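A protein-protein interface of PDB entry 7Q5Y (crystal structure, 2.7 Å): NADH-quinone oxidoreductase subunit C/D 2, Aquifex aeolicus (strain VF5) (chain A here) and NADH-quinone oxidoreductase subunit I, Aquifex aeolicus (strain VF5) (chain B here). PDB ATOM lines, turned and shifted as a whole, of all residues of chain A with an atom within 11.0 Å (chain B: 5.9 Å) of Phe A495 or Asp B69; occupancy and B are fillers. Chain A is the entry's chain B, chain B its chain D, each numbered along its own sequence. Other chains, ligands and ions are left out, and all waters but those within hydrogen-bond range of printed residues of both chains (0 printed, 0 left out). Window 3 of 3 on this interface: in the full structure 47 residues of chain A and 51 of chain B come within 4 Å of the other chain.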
ATOM      1  N   TYR A 353     -16.086   8.267  11.395  1.00  0.00           N
ATOM      2  CA  TYR A 353     -17.388   8.183  10.757  1.00  0.00           C
ATOM      3  C   TYR A 353     -17.848   6.739  10.684  1.00  0.00           C
ATOM      4  O   TYR A 353     -17.091   5.796  10.935  1.00  0.00           O
ATOM      5  CB  TYR A 353     -17.415   8.701   9.307  1.00  0.00           C
ATOM      6  CG  TYR A 353     -16.551   9.865   8.915  1.00  0.00           C
ATOM      7  CD1 TYR A 353     -16.999  11.179   9.097  1.00  0.00           C
ATOM      8  CD2 TYR A 353     -15.329   9.664   8.293  1.00  0.00           C
ATOM      9  CE1 TYR A 353     -16.236  12.259   8.708  1.00  0.00           C
ATOM     10  CE2 TYR A 353     -14.552  10.737   7.903  1.00  0.00           C
ATOM     11  CZ  TYR A 353     -15.011  12.034   8.112  1.00  0.00           C
ATOM     12  OH  TYR A 353     -14.244  13.108   7.718  1.00  0.00           O
ATOM     13  N   LYS A 482     -20.481   8.777  22.857  1.00  0.00           N
ATOM     14  CA  LYS A 482     -20.746  10.178  23.143  1.00  0.00           C
ATOM     15  C   LYS A 482     -21.086  10.453  24.604  1.00  0.00           C
ATOM     16  O   LYS A 482     -21.137  11.622  24.991  1.00  0.00           O
ATOM     17  CB  LYS A 482     -21.895  10.670  22.272  1.00  0.00           C
ATOM     18  CG  LYS A 482     -21.747  10.399  20.790  1.00  0.00           C
ATOM     19  CD  LYS A 482     -22.942  11.033  20.097  1.00  0.00           C
ATOM     20  CE  LYS A 482     -22.977  10.807  18.604  1.00  0.00           C
ATOM     21  NZ  LYS A 482     -24.223  11.446  18.071  1.00  0.00           N
ATOM     22  N   ILE A 488     -14.986  13.873  21.937  1.00  0.00           N
ATOM     23  CA  ILE A 488     -15.458  15.001  21.138  1.00  0.00           C
ATOM     24  C   ILE A 488     -16.613  14.540  20.255  1.00  0.00           C
ATOM     25  O   ILE A 488     -16.454  13.609  19.445  1.00  0.00           O
ATOM     26  CB  ILE A 488     -14.329  15.620  20.293  1.00  0.00           C
ATOM     27  CG1 ILE A 488     -13.240  16.200  21.179  1.00  0.00           C
ATOM     28  CG2 ILE A 488     -14.848  16.661  19.312  1.00  0.00           C
ATOM     29  CD1 ILE A 488     -11.933  16.332  20.469  1.00  0.00           C
ATOM     30  N   PRO A 489     -17.778  15.166  20.370  1.00  0.00           N
ATOM     31  CA  PRO A 489     -18.938  14.770  19.556  1.00  0.00           C
ATOM     32  C   PRO A 489     -18.802  15.236  18.116  1.00  0.00           C
ATOM     33  O   PRO A 489     -18.110  16.228  17.836  1.00  0.00           O
ATOM     34  CB  PRO A 489     -20.114  15.465  20.262  1.00  0.00           C
ATOM     35  CG  PRO A 489     -19.486  16.659  20.933  1.00  0.00           C
ATOM     36  CD  PRO A 489     -18.090  16.239  21.330  1.00  0.00           C
ATOM     37  N   PRO A 490     -19.464  14.556  17.177  1.00  0.00           N
ATOM     38  CA  PRO A 490     -19.391  14.960  15.765  1.00  0.00           C
ATOM     39  C   PRO A 490     -19.984  16.345  15.539  1.00  0.00           C
ATOM     40  O   PRO A 490     -20.854  16.798  16.283  1.00  0.00           O
ATOM     41  CB  PRO A 490     -20.222  13.890  15.045  1.00  0.00           C
ATOM     42  CG  PRO A 490     -21.053  13.240  16.139  1.00  0.00           C
ATOM     43  CD  PRO A 490     -20.222  13.310  17.363  1.00  0.00           C
ATOM     44  N   LYS A 491     -19.509  17.015  14.485  1.00  0.00           N
ATOM     45  CA  LYS A 491     -19.984  18.368  14.200  1.00  0.00           C
ATOM     46  C   LYS A 491     -21.504  18.433  14.089  1.00  0.00           C
ATOM     47  O   LYS A 491     -22.116  19.442  14.464  1.00  0.00           O
ATOM     48  CB  LYS A 491     -19.344  18.917  12.917  1.00  0.00           C
ATOM     49  CG  LYS A 491     -19.313  17.958  11.770  1.00  0.00           C
ATOM     50  CD  LYS A 491     -18.234  18.326  10.775  1.00  0.00           C
ATOM     51  CE  LYS A 491     -18.277  17.400   9.576  1.00  0.00           C
ATOM     52  NZ  LYS A 491     -19.586  17.585   8.898  1.00  0.00           N
ATOM     53  N   GLU A 492     -22.132  17.373  13.579  1.00  0.00           N
ATOM     54  CA  GLU A 492     -23.581  17.381  13.442  1.00  0.00           C
ATOM     55  C   GLU A 492     -24.262  17.578  14.789  1.00  0.00           C
ATOM     56  O   GLU A 492     -25.325  18.213  14.849  1.00  0.00           O
ATOM     57  CB  GLU A 492     -24.054  16.101  12.762  1.00  0.00           C
ATOM     58  CG  GLU A 492     -23.594  15.983  11.313  1.00  0.00           C
ATOM     59  CD  GLU A 492     -22.105  15.674  11.181  1.00  0.00           C
ATOM     60  OE1 GLU A 492     -21.528  15.092  12.130  1.00  0.00           O
ATOM     61  OE2 GLU A 492     -21.512  16.022  10.136  1.00  0.00           O
ATOM     62  N   ASP A 493     -23.666  17.051  15.875  1.00  0.00           N
ATOM     63  CA  ASP A 493     -24.245  17.218  17.209  1.00  0.00           C
ATOM     64  C   ASP A 493     -24.104  18.654  17.687  1.00  0.00           C
ATOM     65  O   ASP A 493     -25.047  19.234  18.236  1.00  0.00           O
ATOM     66  CB  ASP A 493     -23.534  16.338  18.243  1.00  0.00           C
ATOM     67  CG  ASP A 493     -23.827  14.857  18.102  1.00  0.00           C
ATOM     68  OD1 ASP A 493     -24.627  14.456  17.230  1.00  0.00           O
ATOM     69  OD2 ASP A 493     -23.232  14.092  18.902  1.00  0.00           O
ATOM     70  N   VAL A 494     -22.926  19.242  17.473  1.00  0.00           N
ATOM     71  CA  VAL A 494     -22.659  20.605  17.910  1.00  0.00           C
ATOM     72  C   VAL A 494     -23.494  21.614  17.116  1.00  0.00           C
ATOM     73  O   VAL A 494     -23.882  22.659  17.647  1.00  0.00           O
ATOM     74  CB  VAL A 494     -21.144  20.867  17.825  1.00  0.00           C
ATOM     75  CG1 VAL A 494     -20.816  22.276  18.259  1.00  0.00           C
ATOM     76  CG2 VAL A 494     -20.368  19.839  18.670  1.00  0.00           C
ATOM     77  N   PHE A 495     -23.798  21.327  15.848  1.00  0.00           N
ATOM     78  CA  PHE A 495     -24.627  22.240  15.066  1.00  0.00           C
ATOM     79  C   PHE A 495     -26.046  22.279  15.575  1.00  0.00           C
ATOM     80  O   PHE A 495     -26.805  23.171  15.188  1.00  0.00           O
ATOM     81  CB  PHE A 495     -24.778  21.799  13.593  1.00  0.00           C
ATOM     82  CG  PHE A 495     -23.510  21.740  12.798  1.00  0.00           C
ATOM     83  CD1 PHE A 495     -22.391  22.472  13.160  1.00  0.00           C
ATOM     84  CD2 PHE A 495     -23.460  20.967  11.650  1.00  0.00           C
ATOM     85  CE1 PHE A 495     -21.233  22.417  12.399  1.00  0.00           C
ATOM     86  CE2 PHE A 495     -22.309  20.906  10.886  1.00  0.00           C
ATOM     87  CZ  PHE A 495     -21.191  21.637  11.259  1.00  0.00           C
ATOM     88  N   HIS A 496     -26.417  21.296  16.393  1.00  0.00           N
ATOM     89  CA  HIS A 496     -27.762  21.050  16.890  1.00  0.00           C
ATOM     90  C   HIS A 496     -28.078  21.500  18.315  1.00  0.00           C
ATOM     91  O   HIS A 496     -29.147  22.082  18.536  1.00  0.00           O
ATOM     92  CB  HIS A 496     -28.042  19.547  16.773  1.00  0.00           C
ATOM     93  CG  HIS A 496     -29.397  19.155  17.269  1.00  0.00           C
ATOM     94  ND1 HIS A 496     -29.613  18.700  18.550  1.00  0.00           N
ATOM     95  CD2 HIS A 496     -30.615  19.221  16.682  1.00  0.00           C
ATOM     96  CE1 HIS A 496     -30.900  18.462  18.718  1.00  0.00           C
ATOM     97  NE2 HIS A 496     -31.530  18.776  17.601  1.00  0.00           N
ATOM     98  N   ASP A 497     -27.230  21.188  19.299  1.00  0.00           N
ATOM     99  CA  ASP A 497     -27.571  21.512  20.678  1.00  0.00           C
ATOM    100  C   ASP A 497     -26.366  21.953  21.494  1.00  0.00           C
ATOM    101  O   ASP A 497     -25.222  21.578  21.228  1.00  0.00           O
ATOM    102  CB  ASP A 497     -28.242  20.305  21.358  1.00  0.00           C
ATOM    103  CG  ASP A 497     -27.460  18.991  21.166  1.00  0.00           C
ATOM    104  OD1 ASP A 497     -26.441  18.795  21.869  1.00  0.00           O
ATOM    105  OD2 ASP A 497     -27.838  18.171  20.295  1.00  0.00           O
ATOM    106  N   LEU A 498     -26.659  22.765  22.513  1.00  0.00           N
ATOM    107  CA  LEU A 498     -25.615  23.288  23.380  1.00  0.00           C
ATOM    108  C   LEU A 498     -24.980  22.198  24.220  1.00  0.00           C
ATOM    109  O   LEU A 498     -23.784  22.272  24.527  1.00  0.00           O
ATOM    110  CB  LEU A 498     -26.199  24.379  24.270  1.00  0.00           C
ATOM    111  CG  LEU A 498     -25.336  24.847  25.431  1.00  0.00           C
ATOM    112  CD1 LEU A 498     -24.236  25.768  24.929  1.00  0.00           C
ATOM    113  CD2 LEU A 498     -26.213  25.550  26.423  1.00  0.00           C
ATOM    114  N   GLU A 499     -25.763  21.182  24.590  1.00  0.00           N
ATOM    115  CA  GLU A 499     -25.266  20.082  25.413  1.00  0.00           C
ATOM    116  C   GLU A 499     -24.084  19.374  24.754  1.00  0.00           C
ATOM    117  O   GLU A 499     -23.241  18.800  25.450  1.00  0.00           O
ATOM    118  CB  GLU A 499     -26.407  19.114  25.720  1.00  0.00           C
ATOM    119  CG  GLU A 499     -27.554  19.723  26.555  1.00  0.00           C
ATOM    120  CD  GLU A 499     -28.631  20.436  25.727  1.00  0.00           C
ATOM    121  OE1 GLU A 499     -28.378  20.824  24.554  1.00  0.00           O
ATOM    122  OE2 GLU A 499     -29.752  20.606  26.268  1.00  0.00           O
ATOM    123  N   SER A 500     -24.007  19.399  23.416  1.00  0.00           N
ATOM    124  CA  SER A 500     -22.885  18.785  22.718  1.00  0.00           C
ATOM    125  C   SER A 500     -21.773  19.799  22.491  1.00  0.00           C
ATOM    126  O   SER A 500     -20.589  19.475  22.636  1.00  0.00           O
ATOM    127  CB  SER A 500     -23.328  18.206  21.372  1.00  0.00           C
ATOM    128  OG  SER A 500     -24.147  17.056  21.523  1.00  0.00           O
ATOM    129  N   MET A 501     -22.156  21.035  22.178  1.00  0.00           N
ATOM    130  CA  MET A 501     -21.187  22.096  21.927  1.00  0.00           C
ATOM    131  C   MET A 501     -20.211  22.288  23.089  1.00  0.00           C
ATOM    132  O   MET A 501     -18.994  22.385  22.879  1.00  0.00           O
ATOM    133  CB  MET A 501     -21.943  23.389  21.627  1.00  0.00           C
ATOM    134  CG  MET A 501     -21.085  24.607  21.367  1.00  0.00           C
ATOM    135  SD  MET A 501     -21.962  25.747  20.277  1.00  0.00           S
ATOM    136  CE  MET A 501     -22.573  26.830  21.466  1.00  0.00           C
ATOM    137  N   VAL A 502     -20.719  22.341  24.327  1.00  0.00           N
ATOM    138  CA  VAL A 502     -19.834  22.579  25.470  1.00  0.00           C
ATOM    139  C   VAL A 502     -18.785  21.490  25.621  1.00  0.00           C
ATOM    140  O   VAL A 502     -17.703  21.742  26.162  1.00  0.00           O
ATOM    141  CB  VAL A 502     -20.657  22.762  26.751  1.00  0.00           C
ATOM    142  CG1 VAL A 502     -21.695  23.823  26.495  1.00  0.00           C
ATOM    143  CG2 VAL A 502     -21.296  21.426  27.170  1.00  0.00           C
ATOM    144  N   LYS A 503     -19.076  20.274  25.151  1.00  0.00           N
ATOM    145  CA  LYS A 503     -18.089  19.202  25.233  1.00  0.00           C
ATOM    146  C   LYS A 503     -16.952  19.462  24.259  1.00  0.00           C
ATOM    147  O   LYS A 503     -15.775  19.297  24.604  1.00  0.00           O
ATOM    148  CB  LYS A 503     -18.745  17.855  24.949  1.00  0.00           C
ATOM    149  CG  LYS A 503     -19.856  17.470  25.909  1.00  0.00           C
ATOM    150  CD  LYS A 503     -20.296  16.055  25.624  1.00  0.00           C
ATOM    151  CE  LYS A 503     -19.095  15.144  25.612  1.00  0.00           C
ATOM    152  NZ  LYS A 503     -19.494  13.746  25.397  1.00  0.00           N
ATOM    153  N   SER A 504     -17.299  19.865  23.033  1.00  0.00           N
ATOM    154  CA  SER A 504     -16.305  20.172  22.015  1.00  0.00           C
ATOM    155  C   SER A 504     -15.369  21.269  22.495  1.00  0.00           C
ATOM    156  O   SER A 504     -14.141  21.158  22.386  1.00  0.00           O
ATOM    157  CB  SER A 504     -17.016  20.595  20.725  1.00  0.00           C
ATOM    158  OG  SER A 504     -16.114  21.010  19.709  1.00  0.00           O
ATOM    159  N   PHE A 505     -15.940  22.335  23.053  1.00  0.00           N
ATOM    160  CA  PHE A 505     -15.120  23.431  23.531  1.00  0.00           C
ATOM    161  C   PHE A 505     -14.228  22.998  24.680  1.00  0.00           C
ATOM    162  O   PHE A 505     -13.040  23.331  24.708  1.00  0.00           O
ATOM    163  CB  PHE A 505     -16.001  24.612  23.930  1.00  0.00           C
ATOM    164  CG  PHE A 505     -16.304  25.545  22.792  1.00  0.00           C
ATOM    165  CD1 PHE A 505     -17.288  25.231  21.856  1.00  0.00           C
ATOM    166  CD2 PHE A 505     -15.569  26.719  22.627  1.00  0.00           C
ATOM    167  CE1 PHE A 505     -17.569  26.091  20.795  1.00  0.00           C
ATOM    168  CE2 PHE A 505     -15.826  27.581  21.553  1.00  0.00           C
ATOM    169  CZ  PHE A 505     -16.824  27.269  20.637  1.00  0.00           C
ATOM    170  N   GLU B  67     -27.417  27.052   6.256  1.00  0.00           N
ATOM    171  CA  GLU B  67     -26.600  27.064   7.462  1.00  0.00           C
ATOM    172  C   GLU B  67     -27.229  26.252   8.592  1.00  0.00           C
ATOM    173  O   GLU B  67     -28.452  26.110   8.662  1.00  0.00           O
ATOM    174  CB  GLU B  67     -26.375  28.488   7.949  1.00  0.00           C
ATOM    175  CG  GLU B  67     -25.563  29.336   6.989  1.00  0.00           C
ATOM    176  CD  GLU B  67     -26.370  29.790   5.806  1.00  0.00           C
ATOM    177  OE1 GLU B  67     -27.586  30.022   5.984  1.00  0.00           O
ATOM    178  OE2 GLU B  67     -25.798  29.866   4.698  1.00  0.00           O
ATOM    179  N   PRO B  68     -26.404  25.715   9.491  1.00  0.00           N
ATOM    180  CA  PRO B  68     -26.930  24.952  10.628  1.00  0.00           C
ATOM    181  C   PRO B  68     -27.566  25.848  11.690  1.00  0.00           C
ATOM    182  O   PRO B  68     -27.356  27.061  11.754  1.00  0.00           O
ATOM    183  CB  PRO B  68     -25.687  24.245  11.181  1.00  0.00           C
ATOM    184  CG  PRO B  68     -24.545  25.029  10.694  1.00  0.00           C
ATOM    185  CD  PRO B  68     -24.940  25.606   9.381  1.00  0.00           C
ATOM    186  N   ASP B  69     -28.348  25.205  12.558  1.00  0.00           N
ATOM    187  CA  ASP B  69     -29.044  25.931  13.614  1.00  0.00           C
ATOM    188  C   ASP B  69     -28.081  26.734  14.477  1.00  0.00           C
ATOM    189  O   ASP B  69     -28.390  27.862  14.877  1.00  0.00           O
ATOM    190  CB  ASP B  69     -29.831  24.947  14.480  1.00  0.00           C
ATOM    191  CG  ASP B  69     -31.025  24.342  13.761  1.00  0.00           C
ATOM    192  OD1 ASP B  69     -31.132  24.521  12.525  1.00  0.00           O
ATOM    193  OD2 ASP B  69     -31.825  23.645  14.431  1.00  0.00           O
ATOM    194  N   SER B  70     -26.908  26.168  14.777  1.00  0.00           N
ATOM    195  CA  SER B  70     -25.935  26.864  15.617  1.00  0.00           C
ATOM    196  C   SER B  70     -25.507  28.206  15.021  1.00  0.00           C
ATOM    197  O   SER B  70     -25.399  29.201  15.752  1.00  0.00           O
ATOM    198  CB  SER B  70     -24.722  25.978  15.836  1.00  0.00           C
ATOM    199  OG  SER B  70     -24.140  25.649  14.583  1.00  0.00           O
ATOM    200  N   LEU B  71     -25.256  28.262  13.701  1.00  0.00           N
ATOM    201  CA  LEU B  71     -24.855  29.528  13.084  1.00  0.00           C
ATOM    202  C   LEU B  71     -26.037  30.486  12.996  1.00  0.00           C
ATOM    203  O   LEU B  71     -25.917  31.662  13.366  1.00  0.00           O
ATOM    204  CB  LEU B  71     -24.248  29.313  11.692  1.00  0.00           C
ATOM    205  CG  LEU B  71     -23.909  30.604  10.901  1.00  0.00           C
ATOM    206  CD1 LEU B  71     -23.061  31.547  11.711  1.00  0.00           C
ATOM    207  CD2 LEU B  71     -23.216  30.358   9.570  1.00  0.00           C
ATOM    208  N   LYS B  72     -27.194  30.001  12.517  1.00  0.00           N
ATOM    209  CA  LYS B  72     -28.361  30.876  12.433  1.00  0.00           C
ATOM    210  C   LYS B  72     -28.694  31.458  13.797  1.00  0.00           C
ATOM    211  O   LYS B  72     -29.214  32.574  13.890  1.00  0.00           O
ATOM    212  CB  LYS B  72     -29.564  30.131  11.881  1.00  0.00           C
ATOM    213  CG  LYS B  72     -29.391  29.622  10.491  1.00  0.00           C
ATOM    214  CD  LYS B  72     -30.748  29.229   9.892  1.00  0.00           C
ATOM    215  CE  LYS B  72     -31.191  27.873  10.432  1.00  0.00           C
ATOM    216  NZ  LYS B  72     -31.093  26.724   9.470  1.00  0.00           N
ATOM    217  N   ALA B  73     -28.394  30.720  14.863  1.00  0.00           N
ATOM    218  CA  ALA B  73     -28.671  31.205  16.207  1.00  0.00           C
ATOM    219  C   ALA B  73     -27.806  32.407  16.570  1.00  0.00           C
ATOM    220  O   ALA B  73     -28.227  33.238  17.383  1.00  0.00           O
ATOM    221  CB  ALA B  73     -28.468  30.078  17.209  1.00  0.00           C
ATOM    222  N   ILE B  74     -26.608  32.526  15.995  1.00  0.00           N
ATOM    223  CA  ILE B  74     -25.721  33.644  16.301  1.00  0.00           C
ATOM    224  C   ILE B  74     -25.623  34.623  15.145  1.00  0.00           C
ATOM    225  O   ILE B  74     -24.837  35.571  15.209  1.00  0.00           O
ATOM    226  CB  ILE B  74     -24.309  33.187  16.708  1.00  0.00           C
ATOM    227  CG1 ILE B  74     -23.572  32.564  15.536  1.00  0.00           C
ATOM    228  CG2 ILE B  74     -24.336  32.233  17.854  1.00  0.00           C
ATOM    229  CD1 ILE B  74     -22.197  32.082  15.953  1.00  0.00           C
ATOM    230  N   CYS B 137     -15.105  22.792  13.872  1.00  0.00           N
ATOM    231  CA  CYS B 137     -15.931  23.932  13.433  1.00  0.00           C
ATOM    232  C   CYS B 137     -17.377  23.805  13.914  1.00  0.00           C
ATOM    233  O   CYS B 137     -18.102  22.903  13.462  1.00  0.00           O
ATOM    234  CB  CYS B 137     -15.913  24.118  11.933  1.00  0.00           C
ATOM    235  SG  CYS B 137     -16.423  25.802  11.498  1.00  0.00           S
ATOM    236  N   PRO B 138     -17.840  24.691  14.792  1.00  0.00           N
ATOM    237  CA  PRO B 138     -19.205  24.611  15.329  1.00  0.00           C
ATOM    238  C   PRO B 138     -20.278  25.307  14.508  1.00  0.00           C
ATOM    239  O   PRO B 138     -21.452  25.260  14.886  1.00  0.00           O
ATOM    240  CB  PRO B 138     -19.030  25.306  16.680  1.00  0.00           C
ATOM    241  CG  PRO B 138     -18.036  26.444  16.342  1.00  0.00           C
ATOM    242  CD  PRO B 138     -17.112  25.880  15.290  1.00  0.00           C
ATOM    243  N   VAL B 139     -19.903  25.943  13.407  1.00  0.00           N
ATOM    244  CA  VAL B 139     -20.801  26.722  12.572  1.00  0.00           C
ATOM    245  C   VAL B 139     -20.936  26.161  11.152  1.00  0.00           C
ATOM    246  O   VAL B 139     -21.724  26.684  10.350  1.00  0.00           O
ATOM    247  CB  VAL B 139     -20.306  28.192  12.595  1.00  0.00           C
ATOM    248  CG1 VAL B 139     -20.567  28.995  11.347  1.00  0.00           C
ATOM    249  CG2 VAL B 139     -20.884  28.891  13.805  1.00  0.00           C
ATOM    250  N   GLY B 140     -20.241  25.079  10.830  1.00  0.00           N
ATOM    251  CA  GLY B 140     -20.370  24.538   9.483  1.00  0.00           C
ATOM    252  C   GLY B 140     -19.709  25.409   8.435  1.00  0.00           C
ATOM    253  O   GLY B 140     -20.265  25.604   7.346  1.00  0.00           O
ATOM    254  N   CYS B 141     -18.521  25.934   8.743  1.00  0.00           N
ATOM    255  CA  CYS B 141     -17.776  26.798   7.841  1.00  0.00           C
ATOM    256  C   CYS B 141     -16.543  26.104   7.281  1.00  0.00           C
ATOM    257  O   CYS B 141     -16.420  25.974   6.061  1.00  0.00           O
ATOM    258  CB  CYS B 141     -17.365  28.092   8.572  1.00  0.00           C
ATOM    259  SG  CYS B 141     -16.189  29.172   7.653  1.00  0.00           S
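The backbone carbonyl oxygen (O) of Phe A495 lies within hydrogen-bond range of the backbone NH (N) of Ser B70 (3.0 Å).
O of Pro B138 is in hydrogen-bond range of OG of Ser B70 (2.7 Å). The side-chain carboxylate of Asp B69 is in salt-bridge range of the side-chain amino group of Lys B72 (3.8 Å). The side-chain sulfur (SG) of Cys B137 lies close to the backbone NH (N) of Cys B141.
Among the printed residues, merely in contact across the chains: Phe A495 with Gly B140 (3.2 Å), Phe A495 with Cys B137 (3.3 Å), Phe A495 with Pro B138 (3.4 Å), Phe A495 with Pro B68 (3.6 Å), Phe A495 with Asp B69 (3.6 Å), Val A494 with Pro B138 (3.9 Å), Val A494 with Ser B70 (3.9 Å) and Phe A495 with Val B139 (3.9 Å).
Pro A490 touches none of the printed residues of chain B. Of the printed residues of chain B, Val A494 touches Ser B70 (3.9 Å) and Pro B138 (3.9 Å). Printed residues of chain A within 4 Å of Pro B68: Phe A495. Asp B69 touches just one residue of chain A: Phe A495. Ser B70 touches two residues of chain A. Lys B72 touches none of the printed residues of chain A. Cys B137 touches just one residue of chain A: Phe A495 (3.3 Å). Of the printed residues of chain A, Pro B138 touches Val A494 (3.9 Å) and Phe A495 (3.4 Å). Val B139 touches just one residue of chain A: Phe A495. Gly B140 touches just one residue of chain A: Phe A495. The nearest residue of chain B that does not touch Phe A495 is Leu B71 (5.5 Å). The nearest residue of chain A that does not touch Asp B69 is His A496 (5.0 Å).
Of the 13 printed residues of chain B, 7 touch a printed residue of chain A. Printed residues of chain B that touch a printed residue of chain A: Pro B68, Asp B69, Ser B70, Cys B137, Pro B138, Val B139 and Gly B140. Of the 20 printed residues of chain A, 2 touch a printed residue of chain B. Hydrophobic or aromatic side chains of chain A that line the printed part of chain B: Val A494 and Phe A495. Among the printed residues, 9 pairs touch across the chains. Among the printed residues, no Asp or Glu carboxylate lies within 4 Å of a Lys or Arg side-chain nitrogen of the other chain.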
